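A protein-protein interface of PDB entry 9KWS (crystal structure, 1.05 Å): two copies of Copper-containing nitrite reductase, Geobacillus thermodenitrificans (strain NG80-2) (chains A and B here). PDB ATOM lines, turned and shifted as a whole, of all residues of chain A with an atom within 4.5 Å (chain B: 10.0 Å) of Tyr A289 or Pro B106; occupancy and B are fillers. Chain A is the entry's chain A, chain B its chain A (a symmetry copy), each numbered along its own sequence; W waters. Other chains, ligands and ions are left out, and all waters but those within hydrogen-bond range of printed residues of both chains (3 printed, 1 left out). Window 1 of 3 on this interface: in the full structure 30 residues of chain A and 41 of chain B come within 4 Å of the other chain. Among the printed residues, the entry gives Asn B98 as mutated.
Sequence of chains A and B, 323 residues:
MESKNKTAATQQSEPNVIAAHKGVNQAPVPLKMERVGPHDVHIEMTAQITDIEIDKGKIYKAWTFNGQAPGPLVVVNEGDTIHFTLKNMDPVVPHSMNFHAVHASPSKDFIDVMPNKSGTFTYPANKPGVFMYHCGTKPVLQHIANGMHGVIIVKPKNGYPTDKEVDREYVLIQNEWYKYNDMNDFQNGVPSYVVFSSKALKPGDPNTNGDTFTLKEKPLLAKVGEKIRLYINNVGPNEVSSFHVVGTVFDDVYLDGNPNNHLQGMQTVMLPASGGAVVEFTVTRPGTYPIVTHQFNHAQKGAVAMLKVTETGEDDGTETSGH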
ATOM      1  N   VAL A 246      -8.643   9.823 -21.859  1.00  0.00           N
ATOM      2  CA  VAL A 246      -9.613   9.530 -20.814  1.00  0.00           C
ATOM      3  C   VAL A 246      -8.985   8.655 -19.739  1.00  0.00           C
ATOM      4  O   VAL A 246      -8.291   7.686 -20.040  1.00  0.00           O
ATOM      5  CB  VAL A 246     -10.826   8.825 -21.449  1.00  0.00           C
ATOM      6  CG1 VAL A 246     -11.866   8.481 -20.403  1.00  0.00           C
ATOM      7  CG2 VAL A 246     -11.441   9.688 -22.534  1.00  0.00           C
ATOM      8  N   GLY A 247      -9.254   8.974 -18.468  1.00  0.00           N
ATOM      9  CA  GLY A 247      -8.807   8.146 -17.367  1.00  0.00           C
ATOM     10  C   GLY A 247      -7.419   8.439 -16.856  1.00  0.00           C
ATOM     11  O   GLY A 247      -6.922   7.709 -15.982  1.00  0.00           O
ATOM     12  N   VAL A 283      -0.935   5.024 -17.049  1.00  0.00           N
ATOM     13  CA  VAL A 283      -2.156   4.225 -17.045  1.00  0.00           C
ATOM     14  C   VAL A 283      -2.101   3.293 -15.840  1.00  0.00           C
ATOM     15  O   VAL A 283      -1.244   2.412 -15.748  1.00  0.00           O
ATOM     16  CB  VAL A 283      -2.375   3.487 -18.374  1.00  0.00           C
ATOM     17  CG1 VAL A 283      -2.753   4.494 -19.453  1.00  0.00           C
ATOM     18  CG2 VAL A 283      -1.160   2.652 -18.805  1.00  0.00           C
ATOM     19  N   THR A 284      -2.999   3.494 -14.888  1.00  0.00           N
ATOM     20  CA  THR A 284      -2.854   2.858 -13.588  1.00  0.00           C
ATOM     21  C   THR A 284      -3.638   1.567 -13.426  1.00  0.00           C
ATOM     22  O   THR A 284      -3.369   0.827 -12.477  1.00  0.00           O
ATOM     23  CB  THR A 284      -3.303   3.813 -12.478  1.00  0.00           C
ATOM     24  OG1 THR A 284      -4.696   4.112 -12.650  1.00  0.00           O
ATOM     25  CG2 THR A 284      -2.501   5.109 -12.493  1.00  0.00           C
ATOM     26  N   ARG A 285      -4.607   1.294 -14.290  1.00  0.00           N
ATOM     27  CA  ARG A 285      -5.523   0.179 -14.121  1.00  0.00           C
ATOM     28  C   ARG A 285      -5.758  -0.499 -15.462  1.00  0.00           C
ATOM     29  O   ARG A 285      -5.686   0.144 -16.517  1.00  0.00           O
ATOM     30  CB  ARG A 285      -6.872   0.656 -13.556  1.00  0.00           C
ATOM     31  CG  ARG A 285      -6.778   1.147 -12.138  1.00  0.00           C
ATOM     32  CD  ARG A 285      -8.092   1.708 -11.632  1.00  0.00           C
ATOM     33  NE  ARG A 285      -7.947   2.136 -10.249  1.00  0.00           N
ATOM     34  CZ  ARG A 285      -8.897   2.706  -9.528  1.00  0.00           C
ATOM     35  NH1 ARG A 285     -10.096   2.922 -10.022  1.00  0.00           N
ATOM     36  NH2 ARG A 285      -8.632   3.054  -8.276  1.00  0.00           N
ATOM     37  N   GLY A 287      -7.802  -1.838 -18.576  1.00  0.00           N
ATOM     38  CA  GLY A 287      -9.014  -1.431 -19.249  1.00  0.00           C
ATOM     39  C   GLY A 287      -8.688  -0.779 -20.572  1.00  0.00           C
ATOM     40  O   GLY A 287      -7.536  -0.741 -21.007  1.00  0.00           O
ATOM     41  N   THR A 288      -9.731  -0.261 -21.212  1.00  0.00           N
ATOM     42  CA  THR A 288      -9.582   0.452 -22.472  1.00  0.00           C
ATOM     43  C   THR A 288      -9.807   1.932 -22.223  1.00  0.00           C
ATOM     44  O   THR A 288     -10.799   2.323 -21.595  1.00  0.00           O
ATOM     45  CB  THR A 288     -10.501  -0.119 -23.544  1.00  0.00           C
ATOM     46  OG1 THR A 288     -10.135  -1.487 -23.769  1.00  0.00           O
ATOM     47  CG2 THR A 288     -10.342   0.644 -24.848  1.00  0.00           C
ATOM     48  N   TYR A 289      -8.864   2.735 -22.703  1.00  0.00           N
ATOM     49  CA  TYR A 289      -8.791   4.165 -22.461  1.00  0.00           C
ATOM     50  C   TYR A 289      -9.008   4.892 -23.779  1.00  0.00           C
ATOM     51  O   TYR A 289      -8.133   4.836 -24.662  1.00  0.00           O
ATOM     52  CB  TYR A 289      -7.418   4.547 -21.913  1.00  0.00           C
ATOM     53  CG  TYR A 289      -7.078   4.055 -20.525  1.00  0.00           C
ATOM     54  CD1 TYR A 289      -6.957   2.703 -20.240  1.00  0.00           C
ATOM     55  CD2 TYR A 289      -6.856   4.952 -19.489  1.00  0.00           C
ATOM     56  CE1 TYR A 289      -6.650   2.268 -18.959  1.00  0.00           C
ATOM     57  CE2 TYR A 289      -6.533   4.526 -18.222  1.00  0.00           C
ATOM     58  CZ  TYR A 289      -6.422   3.184 -17.961  1.00  0.00           C
ATOM     59  OH  TYR A 289      -6.096   2.775 -16.679  1.00  0.00           O
ATOM     60  N   PRO A 290     -10.119   5.602 -23.952  1.00  0.00           N
ATOM     61  CA  PRO A 290     -10.279   6.408 -25.165  1.00  0.00           C
ATOM     62  C   PRO A 290      -9.301   7.571 -25.203  1.00  0.00           C
ATOM     63  O   PRO A 290      -8.896   8.125 -24.173  1.00  0.00           O
ATOM     64  CB  PRO A 290     -11.737   6.885 -25.085  1.00  0.00           C
ATOM     65  CG  PRO A 290     -12.413   5.879 -24.185  1.00  0.00           C
ATOM     66  CD  PRO A 290     -11.366   5.529 -23.172  1.00  0.00           C
ATOM     67  N   ILE A 291      -8.954   7.950 -26.428  1.00  0.00           N
ATOM     68  CA  ILE A 291      -8.103   9.082 -26.751  1.00  0.00           C
ATOM     69  C   ILE A 291      -8.914   9.949 -27.702  1.00  0.00           C
ATOM     70  O   ILE A 291      -9.381   9.456 -28.736  1.00  0.00           O
ATOM     71  CB  ILE A 291      -6.796   8.618 -27.421  1.00  0.00           C
ATOM     72  CG1 ILE A 291      -6.011   7.671 -26.499  1.00  0.00           C
ATOM     73  CG2 ILE A 291      -5.962   9.829 -27.825  1.00  0.00           C
ATOM     74  CD1 ILE A 291      -4.859   6.977 -27.182  1.00  0.00           C
ATOM     75  N   ALA A 305      -9.620   7.369 -30.674  1.00  0.00           N
ATOM     76  CA  ALA A 305      -8.759   6.199 -30.746  1.00  0.00           C
ATOM     77  C   ALA A 305      -8.841   5.495 -29.396  1.00  0.00           C
ATOM     78  O   ALA A 305      -9.399   6.036 -28.444  1.00  0.00           O
ATOM     79  CB  ALA A 305      -7.320   6.612 -31.074  1.00  0.00           C
ATOM     80  N   MET A 306      -8.323   4.271 -29.311  1.00  0.00           N
ATOM     81  CA  MET A 306      -8.387   3.514 -28.069  1.00  0.00           C
ATOM     82  C   MET A 306      -7.014   2.974 -27.699  1.00  0.00           C
ATOM     83  O   MET A 306      -6.237   2.566 -28.570  1.00  0.00           O
ATOM     84  CB  MET A 306      -9.382   2.349 -28.194  1.00  0.00           C
ATOM     85  CG  MET A 306     -10.800   2.776 -28.530  1.00  0.00           C
ATOM     86  SD  MET A 306     -11.627   3.638 -27.188  1.00  0.00           S
ATOM     87  CE  MET A 306     -13.255   3.861 -27.853  1.00  0.00           C
ATOM     88  N   LEU A 307      -6.742   2.951 -26.393  1.00  0.00           N
ATOM     89  CA  LEU A 307      -5.538   2.369 -25.803  1.00  0.00           C
ATOM     90  C   LEU A 307      -5.989   1.262 -24.854  1.00  0.00           C
ATOM     91  O   LEU A 307      -6.656   1.534 -23.852  1.00  0.00           O
ATOM     92  CB  LEU A 307      -4.764   3.446 -25.050  1.00  0.00           C
ATOM     93  CG  LEU A 307      -3.536   2.992 -24.275  1.00  0.00           C
ATOM     94  CD1 LEU A 307      -2.447   2.467 -25.206  1.00  0.00           C
ATOM     95  CD2 LEU A 307      -3.008   4.135 -23.436  1.00  0.00           C
ATOM     96  N   VAL A 309      -5.105  -1.453 -22.166  1.00  0.00           N
ATOM     97  CA  VAL A 309      -4.098  -1.614 -21.128  1.00  0.00           C
ATOM     98  C   VAL A 309      -4.376  -2.942 -20.441  1.00  0.00           C
ATOM     99  O   VAL A 309      -5.445  -3.135 -19.851  1.00  0.00           O
ATOM    100  CB  VAL A 309      -4.148  -0.440 -20.137  1.00  0.00           C
ATOM    101  CG1 VAL A 309      -3.111  -0.593 -19.050  1.00  0.00           C
ATOM    102  CG2 VAL A 309      -3.968   0.889 -20.877  1.00  0.00           C
ATOM    103  N   SER B  96     -23.449   8.116 -16.802  1.00  0.00           N
ATOM    104  CA  SER B  96     -22.181   7.731 -16.212  1.00  0.00           C
ATOM    105  C   SER B  96     -21.447   8.992 -15.775  1.00  0.00           C
ATOM    106  O   SER B  96     -21.944  10.107 -15.922  1.00  0.00           O
ATOM    107  CB  SER B  96     -21.341   6.943 -17.212  1.00  0.00           C
ATOM    108  OG  SER B  96     -21.085   7.716 -18.376  1.00  0.00           O
ATOM    109  N   MET B  97     -20.247   8.802 -15.234  1.00  0.00           N
ATOM    110  CA  MET B  97     -19.397   9.894 -14.774  1.00  0.00           C
ATOM    111  C   MET B  97     -17.952   9.689 -15.151  1.00  0.00           C
ATOM    112  O   MET B  97     -17.362   8.656 -14.828  1.00  0.00           O
ATOM    113  CB  MET B  97     -19.506  10.091 -13.264  1.00  0.00           C
ATOM    114  CG  MET B  97     -18.611  11.192 -12.714  1.00  0.00           C
ATOM    115  SD  MET B  97     -18.855  12.824 -13.339  1.00  0.00           S
ATOM    116  CE  MET B  97     -20.196  13.332 -12.210  1.00  0.00           C
ATOM    117  N   ASN B  98     -17.381  10.707 -15.792  1.00  0.00           N
ATOM    118  CA  ASN B  98     -15.961  10.805 -16.127  1.00  0.00           C
ATOM    119  C   ASN B  98     -15.462  12.066 -15.425  1.00  0.00           C
ATOM    120  O   ASN B  98     -15.918  13.169 -15.731  1.00  0.00           O
ATOM    121  CB  ASN B  98     -15.861  10.962 -17.645  1.00  0.00           C
ATOM    122  CG  ASN B  98     -14.459  11.215 -18.150  1.00  0.00           C
ATOM    123  OD1 ASN B  98     -13.619  11.765 -17.463  1.00  0.00           O
ATOM    124  ND2 ASN B  98     -14.246  10.910 -19.425  1.00  0.00           N
ATOM    125  N   PHE B  99     -14.558  11.912 -14.457  1.00  0.00           N
ATOM    126  CA  PHE B  99     -13.870  13.051 -13.859  1.00  0.00           C
ATOM    127  C   PHE B  99     -12.496  13.185 -14.514  1.00  0.00           C
ATOM    128  O   PHE B  99     -11.687  12.254 -14.430  1.00  0.00           O
ATOM    129  CB  PHE B  99     -13.627  12.846 -12.359  1.00  0.00           C
ATOM    130  CG  PHE B  99     -14.851  12.919 -11.473  1.00  0.00           C
ATOM    131  CD1 PHE B  99     -15.418  14.132 -11.121  1.00  0.00           C
ATOM    132  CD2 PHE B  99     -15.381  11.764 -10.924  1.00  0.00           C
ATOM    133  CE1 PHE B  99     -16.514  14.191 -10.288  1.00  0.00           C
ATOM    134  CE2 PHE B  99     -16.473  11.821 -10.076  1.00  0.00           C
ATOM    135  CZ  PHE B  99     -17.037  13.028  -9.753  1.00  0.00           C
ATOM    136  N   HIS B 100     -12.191  14.344 -15.109  1.00  0.00           N
ATOM    137  CA  HIS B 100     -10.851  14.525 -15.672  1.00  0.00           C
ATOM    138  C   HIS B 100      -9.774  14.564 -14.595  1.00  0.00           C
ATOM    139  O   HIS B 100      -8.591  14.419 -14.904  1.00  0.00           O
ATOM    140  CB  HIS B 100     -10.775  15.807 -16.489  1.00  0.00           C
ATOM    141  CG  HIS B 100     -11.428  15.713 -17.826  1.00  0.00           C
ATOM    142  ND1 HIS B 100     -11.166  16.631 -18.814  1.00  0.00           N
ATOM    143  CD2 HIS B 100     -12.285  14.813 -18.368  1.00  0.00           C
ATOM    144  CE1 HIS B 100     -11.846  16.307 -19.903  1.00  0.00           C
ATOM    145  NE2 HIS B 100     -12.532  15.201 -19.667  1.00  0.00           N
ATOM    146  N   VAL B 102      -9.171  12.390 -12.275  1.00  0.00           N
ATOM    147  CA  VAL B 102      -8.787  11.130 -11.670  1.00  0.00           C
ATOM    148  C   VAL B 102      -8.020  10.231 -12.621  1.00  0.00           C
ATOM    149  O   VAL B 102      -8.132  10.308 -13.846  1.00  0.00           O
ATOM    150  CB  VAL B 102      -9.990  10.369 -11.056  1.00  0.00           C
ATOM    151  CG1 VAL B 102     -10.718  11.256 -10.063  1.00  0.00           C
ATOM    152  CG2 VAL B 102     -10.922   9.826 -12.132  1.00  0.00           C
ATOM    153  N   HIS B 103      -7.255   9.324 -12.016  1.00  0.00           N
ATOM    154  CA  HIS B 103      -6.685   8.170 -12.702  1.00  0.00           C
ATOM    155  C   HIS B 103      -7.618   6.986 -12.494  1.00  0.00           C
ATOM    156  O   HIS B 103      -7.847   6.563 -11.352  1.00  0.00           O
ATOM    157  CB  HIS B 103      -5.297   7.829 -12.173  1.00  0.00           C
ATOM    158  CG  HIS B 103      -4.238   8.732 -12.687  1.00  0.00           C
ATOM    159  ND1 HIS B 103      -3.964   9.956 -12.118  1.00  0.00           N
ATOM    160  CD2 HIS B 103      -3.409   8.602 -13.748  1.00  0.00           C
ATOM    161  CE1 HIS B 103      -2.985  10.527 -12.803  1.00  0.00           C
ATOM    162  NE2 HIS B 103      -2.634   9.729 -13.800  1.00  0.00           N
ATOM    163  N   ALA B 104      -8.170   6.466 -13.582  1.00  0.00           N
ATOM    164  CA  ALA B 104      -9.167   5.415 -13.506  1.00  0.00           C
ATOM    165  C   ALA B 104      -9.127   4.583 -14.775  1.00  0.00           C
ATOM    166  O   ALA B 104      -8.605   5.019 -15.800  1.00  0.00           O
ATOM    167  CB  ALA B 104     -10.561   6.017 -13.339  1.00  0.00           C
ATOM    168  N   SER B 105      -9.708   3.380 -14.699  1.00  0.00           N
ATOM    169  CA  SER B 105      -9.925   2.561 -15.887  1.00  0.00           C
ATOM    170  C   SER B 105     -11.241   2.988 -16.510  1.00  0.00           C
ATOM    171  O   SER B 105     -12.292   2.753 -15.904  1.00  0.00           O
ATOM    172  CB  SER B 105     -10.021   1.098 -15.500  1.00  0.00           C
ATOM    173  OG  SER B 105     -10.567   0.368 -16.583  1.00  0.00           O
ATOM    174  N   PRO B 106     -11.259   3.595 -17.700  1.00  0.00           N
ATOM    175  CA  PRO B 106     -12.553   4.086 -18.202  1.00  0.00           C
ATOM    176  C   PRO B 106     -13.578   2.987 -18.393  1.00  0.00           C
ATOM    177  O   PRO B 106     -14.769   3.192 -18.119  1.00  0.00           O
ATOM    178  CB  PRO B 106     -12.175   4.818 -19.492  1.00  0.00           C
ATOM    179  CG  PRO B 106     -10.773   5.294 -19.209  1.00  0.00           C
ATOM    180  CD  PRO B 106     -10.138   4.114 -18.505  1.00  0.00           C
ATOM    181  N   SER B 107     -13.148   1.814 -18.847  1.00  0.00           N
ATOM    182  CA  SER B 107     -14.052   0.711 -19.146  1.00  0.00           C
ATOM    183  C   SER B 107     -14.507  -0.058 -17.915  1.00  0.00           C
ATOM    184  O   SER B 107     -15.358  -0.938 -18.043  1.00  0.00           O
ATOM    185  CB  SER B 107     -13.380  -0.226 -20.149  1.00  0.00           C
ATOM    186  OG  SER B 107     -12.117  -0.638 -19.667  1.00  0.00           O
ATOM    187  N   LYS B 108     -13.973   0.249 -16.739  1.00  0.00           N
ATOM    188  CA  LYS B 108     -14.448  -0.327 -15.490  1.00  0.00           C
ATOM    189  C   LYS B 108     -15.036   0.705 -14.544  1.00  0.00           C
ATOM    190  O   LYS B 108     -15.969   0.387 -13.800  1.00  0.00           O
ATOM    191  CB  LYS B 108     -13.301  -1.053 -14.770  1.00  0.00           C
ATOM    192  CG  LYS B 108     -12.716  -2.214 -15.555  1.00  0.00           C
ATOM    193  CD  LYS B 108     -11.498  -2.812 -14.861  1.00  0.00           C
ATOM    194  CE  LYS B 108     -11.023  -4.083 -15.547  1.00  0.00           C
ATOM    195  NZ  LYS B 108     -10.246  -4.938 -14.607  1.00  0.00           N
ATOM    196  N   ASP B 109     -14.521   1.934 -14.558  1.00  0.00           N
ATOM    197  CA  ASP B 109     -14.845   2.926 -13.552  1.00  0.00           C
ATOM    198  C   ASP B 109     -15.724   4.062 -14.044  1.00  0.00           C
ATOM    199  O   ASP B 109     -16.276   4.783 -13.209  1.00  0.00           O
ATOM    200  CB  ASP B 109     -13.552   3.541 -12.994  1.00  0.00           C
ATOM    201  CG  ASP B 109     -12.624   2.532 -12.353  1.00  0.00           C
ATOM    202  OD1 ASP B 109     -13.122   1.596 -11.697  1.00  0.00           O
ATOM    203  OD2 ASP B 109     -11.390   2.691 -12.479  1.00  0.00           O
ATOM    204  N   PHE B 110     -15.816   4.272 -15.361  1.00  0.00           N
ATOM    205  CA  PHE B 110     -16.648   5.314 -15.952  1.00  0.00           C
ATOM    206  C   PHE B 110     -17.826   4.680 -16.704  1.00  0.00           C
ATOM    207  O   PHE B 110     -18.308   5.219 -17.700  1.00  0.00           O
ATOM    208  CB  PHE B 110     -15.856   6.220 -16.903  1.00  0.00           C
ATOM    209  CG  PHE B 110     -14.719   7.029 -16.292  1.00  0.00           C
ATOM    210  CD1 PHE B 110     -14.549   7.223 -14.931  1.00  0.00           C
ATOM    211  CD2 PHE B 110     -13.845   7.676 -17.155  1.00  0.00           C
ATOM    212  CE1 PHE B 110     -13.511   8.013 -14.443  1.00  0.00           C
ATOM    213  CE2 PHE B 110     -12.819   8.472 -16.678  1.00  0.00           C
ATOM    214  CZ  PHE B 110     -12.648   8.648 -15.320  1.00  0.00           C
ATOM    215  N   ILE B 111     -18.334   3.556 -16.210  1.00  0.00           N
ATOM    216  CA  ILE B 111     -19.344   2.779 -16.915  1.00  0.00           C
ATOM    217  C   ILE B 111     -20.764   3.247 -16.601  1.00  0.00           C
ATOM    218  O   ILE B 111     -21.022   4.015 -15.661  1.00  0.00           O
ATOM    219  CB  ILE B 111     -19.197   1.274 -16.615  1.00  0.00           C
ATOM    220  CG1 ILE B 111     -19.314   0.984 -15.113  1.00  0.00           C
ATOM    221  CG2 ILE B 111     -17.863   0.791 -17.161  1.00  0.00           C
ATOM    222  CD1 ILE B 111     -19.453  -0.490 -14.800  1.00  0.00           C
ATOM    223  N   ASP B 112     -21.700   2.769 -17.403  1.00  0.00           N
ATOM    224  CA  ASP B 112     -23.072   3.227 -17.329  1.00  0.00           C
ATOM    225  C   ASP B 112     -23.789   2.709 -16.089  1.00  0.00           C
ATOM    226  O   ASP B 112     -23.574   1.582 -15.630  1.00  0.00           O
ATOM    227  CB  ASP B 112     -23.834   2.803 -18.585  1.00  0.00           C
ATOM    228  CG  ASP B 112     -23.352   3.523 -19.841  1.00  0.00           C
ATOM    229  OD1 ASP B 112     -22.707   4.584 -19.729  1.00  0.00           O
ATOM    230  OD2 ASP B 112     -23.606   3.014 -20.956  1.00  0.00           O
ATOM    231  N   PHE B 121     -18.079   4.028  -7.705  1.00  0.00           N
ATOM    232  CA  PHE B 121     -16.793   3.938  -8.379  1.00  0.00           C
ATOM    233  C   PHE B 121     -15.779   4.705  -7.550  1.00  0.00           C
ATOM    234  O   PHE B 121     -16.083   5.787  -7.045  1.00  0.00           O
ATOM    235  CB  PHE B 121     -16.909   4.575  -9.771  1.00  0.00           C
ATOM    236  CG  PHE B 121     -18.086   4.074 -10.535  1.00  0.00           C
ATOM    237  CD1 PHE B 121     -18.047   2.832 -11.134  1.00  0.00           C
ATOM    238  CD2 PHE B 121     -19.265   4.798 -10.596  1.00  0.00           C
ATOM    239  CE1 PHE B 121     -19.143   2.337 -11.806  1.00  0.00           C
ATOM    240  CE2 PHE B 121     -20.359   4.304 -11.276  1.00  0.00           C
ATOM    241  CZ  PHE B 121     -20.294   3.080 -11.877  1.00  0.00           C
ATOM    242  N   THR B 122     -14.565   4.161  -7.425  1.00  0.00           N
ATOM    243  CA  THR B 122     -13.551   4.757  -6.559  1.00  0.00           C
ATOM    244  C   THR B 122     -12.268   5.000  -7.332  1.00  0.00           C
ATOM    245  O   THR B 122     -11.808   4.128  -8.077  1.00  0.00           O
ATOM    246  CB  THR B 122     -13.301   3.858  -5.344  1.00  0.00           C
ATOM    247  OG1 THR B 122     -14.526   3.710  -4.611  1.00  0.00           O
ATOM    248  CG2 THR B 122     -12.223   4.451  -4.454  1.00  0.00           C
ATOM    249  N   TYR B 123     -11.682   6.184  -7.150  1.00  0.00           N
ATOM    250  CA  TYR B 123     -10.494   6.545  -7.909  1.00  0.00           C
ATOM    251  C   TYR B 123      -9.817   7.755  -7.276  1.00  0.00           C
ATOM    252  O   TYR B 123     -10.486   8.611  -6.673  1.00  0.00           O
ATOM    253  CB  TYR B 123     -10.810   6.815  -9.394  1.00  0.00           C
ATOM    254  CG  TYR B 123     -12.242   7.237  -9.682  1.00  0.00           C
ATOM    255  CD1 TYR B 123     -12.819   8.330  -9.040  1.00  0.00           C
ATOM    256  CD2 TYR B 123     -13.021   6.542 -10.594  1.00  0.00           C
ATOM    257  CE1 TYR B 123     -14.122   8.702  -9.297  1.00  0.00           C
ATOM    258  CE2 TYR B 123     -14.321   6.914 -10.876  1.00  0.00           C
ATOM    259  CZ  TYR B 123     -14.873   8.006 -10.215  1.00  0.00           C
ATOM    260  OH  TYR B 123     -16.165   8.407 -10.444  1.00  0.00           O
ATOM    261  N   PRO B 124      -8.500   7.870  -7.429  1.00  0.00           N
ATOM    262  CA  PRO B 124      -7.747   8.970  -6.823  1.00  0.00           C
ATOM    263  C   PRO B 124      -7.648  10.208  -7.700  1.00  0.00           C
ATOM    264  O   PRO B 124      -7.532  10.126  -8.925  1.00  0.00           O
ATOM    265  CB  PRO B 124      -6.350   8.354  -6.657  1.00  0.00           C
ATOM    266  CG  PRO B 124      -6.236   7.443  -7.843  1.00  0.00           C
ATOM    267  CD  PRO B 124      -7.607   6.842  -8.006  1.00  0.00           C
ATOM    268  N   HIS B 134     -17.941  15.087 -16.643  1.00  0.00           N
ATOM    269  CA  HIS B 134     -19.070  14.991 -17.551  1.00  0.00           C
ATOM    270  C   HIS B 134     -19.557  13.556 -17.619  1.00  0.00           C
ATOM    271  O   HIS B 134     -18.839  12.621 -17.276  1.00  0.00           O
ATOM    272  CB  HIS B 134     -18.709  15.488 -18.959  1.00  0.00           C
ATOM    273  CG  HIS B 134     -17.561  14.760 -19.585  1.00  0.00           C
ATOM    274  ND1 HIS B 134     -17.717  13.604 -20.319  1.00  0.00           N
ATOM    275  CD2 HIS B 134     -16.232  15.037 -19.612  1.00  0.00           C
ATOM    276  CE1 HIS B 134     -16.535  13.210 -20.775  1.00  0.00           C
ATOM    277  NE2 HIS B 134     -15.613  14.056 -20.355  1.00  0.00           N
ATOM    278  N   GLY B 136     -20.102  10.170 -19.464  1.00  0.00           N
ATOM    279  CA  GLY B 136     -19.313   9.465 -20.449  1.00  0.00           C
ATOM    280  C   GLY B 136     -20.058   8.402 -21.226  1.00  0.00           C
ATOM    281  O   GLY B 136     -19.435   7.485 -21.758  1.00  0.00           O
ATOM    282  N   THR B 137     -21.380   8.504 -21.312  1.00  0.00           N
ATOM    283  CA  THR B 137     -22.207   7.515 -21.990  1.00  0.00           C
ATOM    284  C   THR B 137     -22.270   7.823 -23.483  1.00  0.00           C
ATOM    285  O   THR B 137     -22.421   8.976 -23.894  1.00  0.00           O
ATOM    286  CB  THR B 137     -23.596   7.519 -21.350  1.00  0.00           C
ATOM    287  OG1 THR B 137     -23.463   7.170 -19.959  1.00  0.00           O
ATOM    288  CG2 THR B 137     -24.554   6.550 -22.019  1.00  0.00           C
ATOM    289  N   VAL B 140     -21.117  10.399 -26.391  1.00  0.00           N
ATOM    290  CA  VAL B 140     -20.727  11.353 -25.359  1.00  0.00           C
ATOM    291  C   VAL B 140     -21.111  12.770 -25.755  1.00  0.00           C
ATOM    292  O   VAL B 140     -21.551  13.556 -24.914  1.00  0.00           O
ATOM    293  CB  VAL B 140     -19.229  11.202 -25.037  1.00  0.00           C
ATOM    294  CG1 VAL B 140     -18.763  12.277 -24.083  1.00  0.00           C
ATOM    295  CG2 VAL B 140     -18.966   9.824 -24.447  1.00  0.00           C
HETATM  296  O   HOH W   1      -5.573   5.059 -10.185  1.00  0.00           O
HETATM  297  O   HOH W   2     -10.974  11.646 -18.426  1.00  0.00           O
HETATM  298  O   HOH W   3      -9.324   4.029  -5.679  1.00  0.00           O
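The backbone NH of Val A309 is in hydrogen-bond range of the backbone carbonyl oxygen of Gly A287 (2.8 Å).
The backbone NH (N) of Ser B105 lies within hydrogen-bond range of the side-chain carboxylate (OD2) of Asp B109, at 2.9 Å.
N of Tyr A289 sits at hydrogen-bond distance from O of Leu A307, at 2.8 Å.
The backbone carbonyl oxygen (O) of Arg A285 lies within hydrogen-bond range of the side-chain hydroxyl (OH) of Tyr A289.
No position is printed for both chains.
Of the 21 pairs that touch across the chains among the printed residues, none has its exchanged pair printed and touching as well.
Val A246 touches Asn B98.
Val A246 touches Phe B110.
Val B102 touches Gly A247.
Gly A247 touches Pro B106.
CB of His B103 touches OG1 of Thr A284, at 3.8 Å.
Arg A285 touches Tyr B123 (NH2 to CA, 3.97 Å).
Arg A285 touches Pro B124.
OG of Ser B105 touches CA of Gly A287, 3.6 Å away.
OH of Tyr A289 touches CA of Ser B105 (3.9 Å).
Tyr A289 touches Pro B106 (CD2 to CD, 3.5 Å).
Printed residues of chain A that touch a printed residue of chain B: Val A246, Gly A247, Thr A284, Arg A285, Gly A287, Thr A288, Tyr A289 and Pro A290.
Hydrophobic or aromatic side chains of chain A within 4 Å of the printed part of chain B: Val A246, Tyr A289 and Pro A290.
Hydrophobic or aromatic side chains of chain B within 4 Å of the printed part of chain A: His B103, Pro B106, Phe B110 and Pro B124.
Among the printed residues, Asp or Glu carboxylates within 4 Å of a Lys or Arg side-chain nitrogen of the other chain: Arg A285 with Asp B109 (2.8 Å).
Printed residues of chain A within 4 Å of Pro B106: Val A246, Gly A247, Thr A288, Tyr A289 and Pro A290.
Of chain B, only Asn B98 (3.5 Å), Pro B106 (3.5 Å) and Phe B110 (3.8 Å) come within 4 Å of Val A246.
No residue of chain B comes within 4 Å of Val A283.
Thr A288 touches just these residues of chain B: Pro B106 (3.5 Å) and Ser B107 (2.9 Å).
Of chain B, only Pro B106 (3.8 Å) comes within 4 Å of Pro A290.
No residue of chain B comes within 4 Å of Val A309.
Of the printed residues of chain A, Phe B110 touches Val A246.
Printed residues of chain B within 4 Å of Arg A285: Ser B105 (3.7 Å), Asp B109 (2.8 Å), Thr B122 (2.9 Å), Tyr B123 (3.97 Å) and Pro B124 (3.9 Å).
The nearest printed residue of chain A that does not touch Ser B107 is Tyr A289 (5.6 Å).
The side-chain hydroxyl of Tyr A289 lies close to the backbone carbonyl oxygen of Ala B104, at 3.5 Å.
OD2 of Asp B109 is in salt-bridge range of NH1 of Arg A285 (2.8 Å).
The guanidinium group (NH1) of Arg A285 sits at hydrogen-bond distance from the backbone carbonyl oxygen (O) of Thr B122 (2.9 Å).
The backbone NH of Thr A288 sits at hydrogen-bond distance from the side-chain hydroxyl of Ser B107.
The backbone NH (N) of Ala B104 sits at hydrogen-bond distance from the backbone carbonyl oxygen (O) of Gly A247 (3.0 Å).
Water W1 bridges the side-chain hydroxyl (OG1) of Thr A284 (2.8 Å) and the backbone carbonyl oxygen (O) of His B103 (3.0 Å).
Water W2 bridges the side-chain amide oxygen of Asn B98 and the backbone NH of Gly A247.
Water W3 bridges the guanidinium group (NH2) of Arg A285 (2.9 Å) and the backbone carbonyl oxygen (O) of Thr B122 (3.5 Å).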
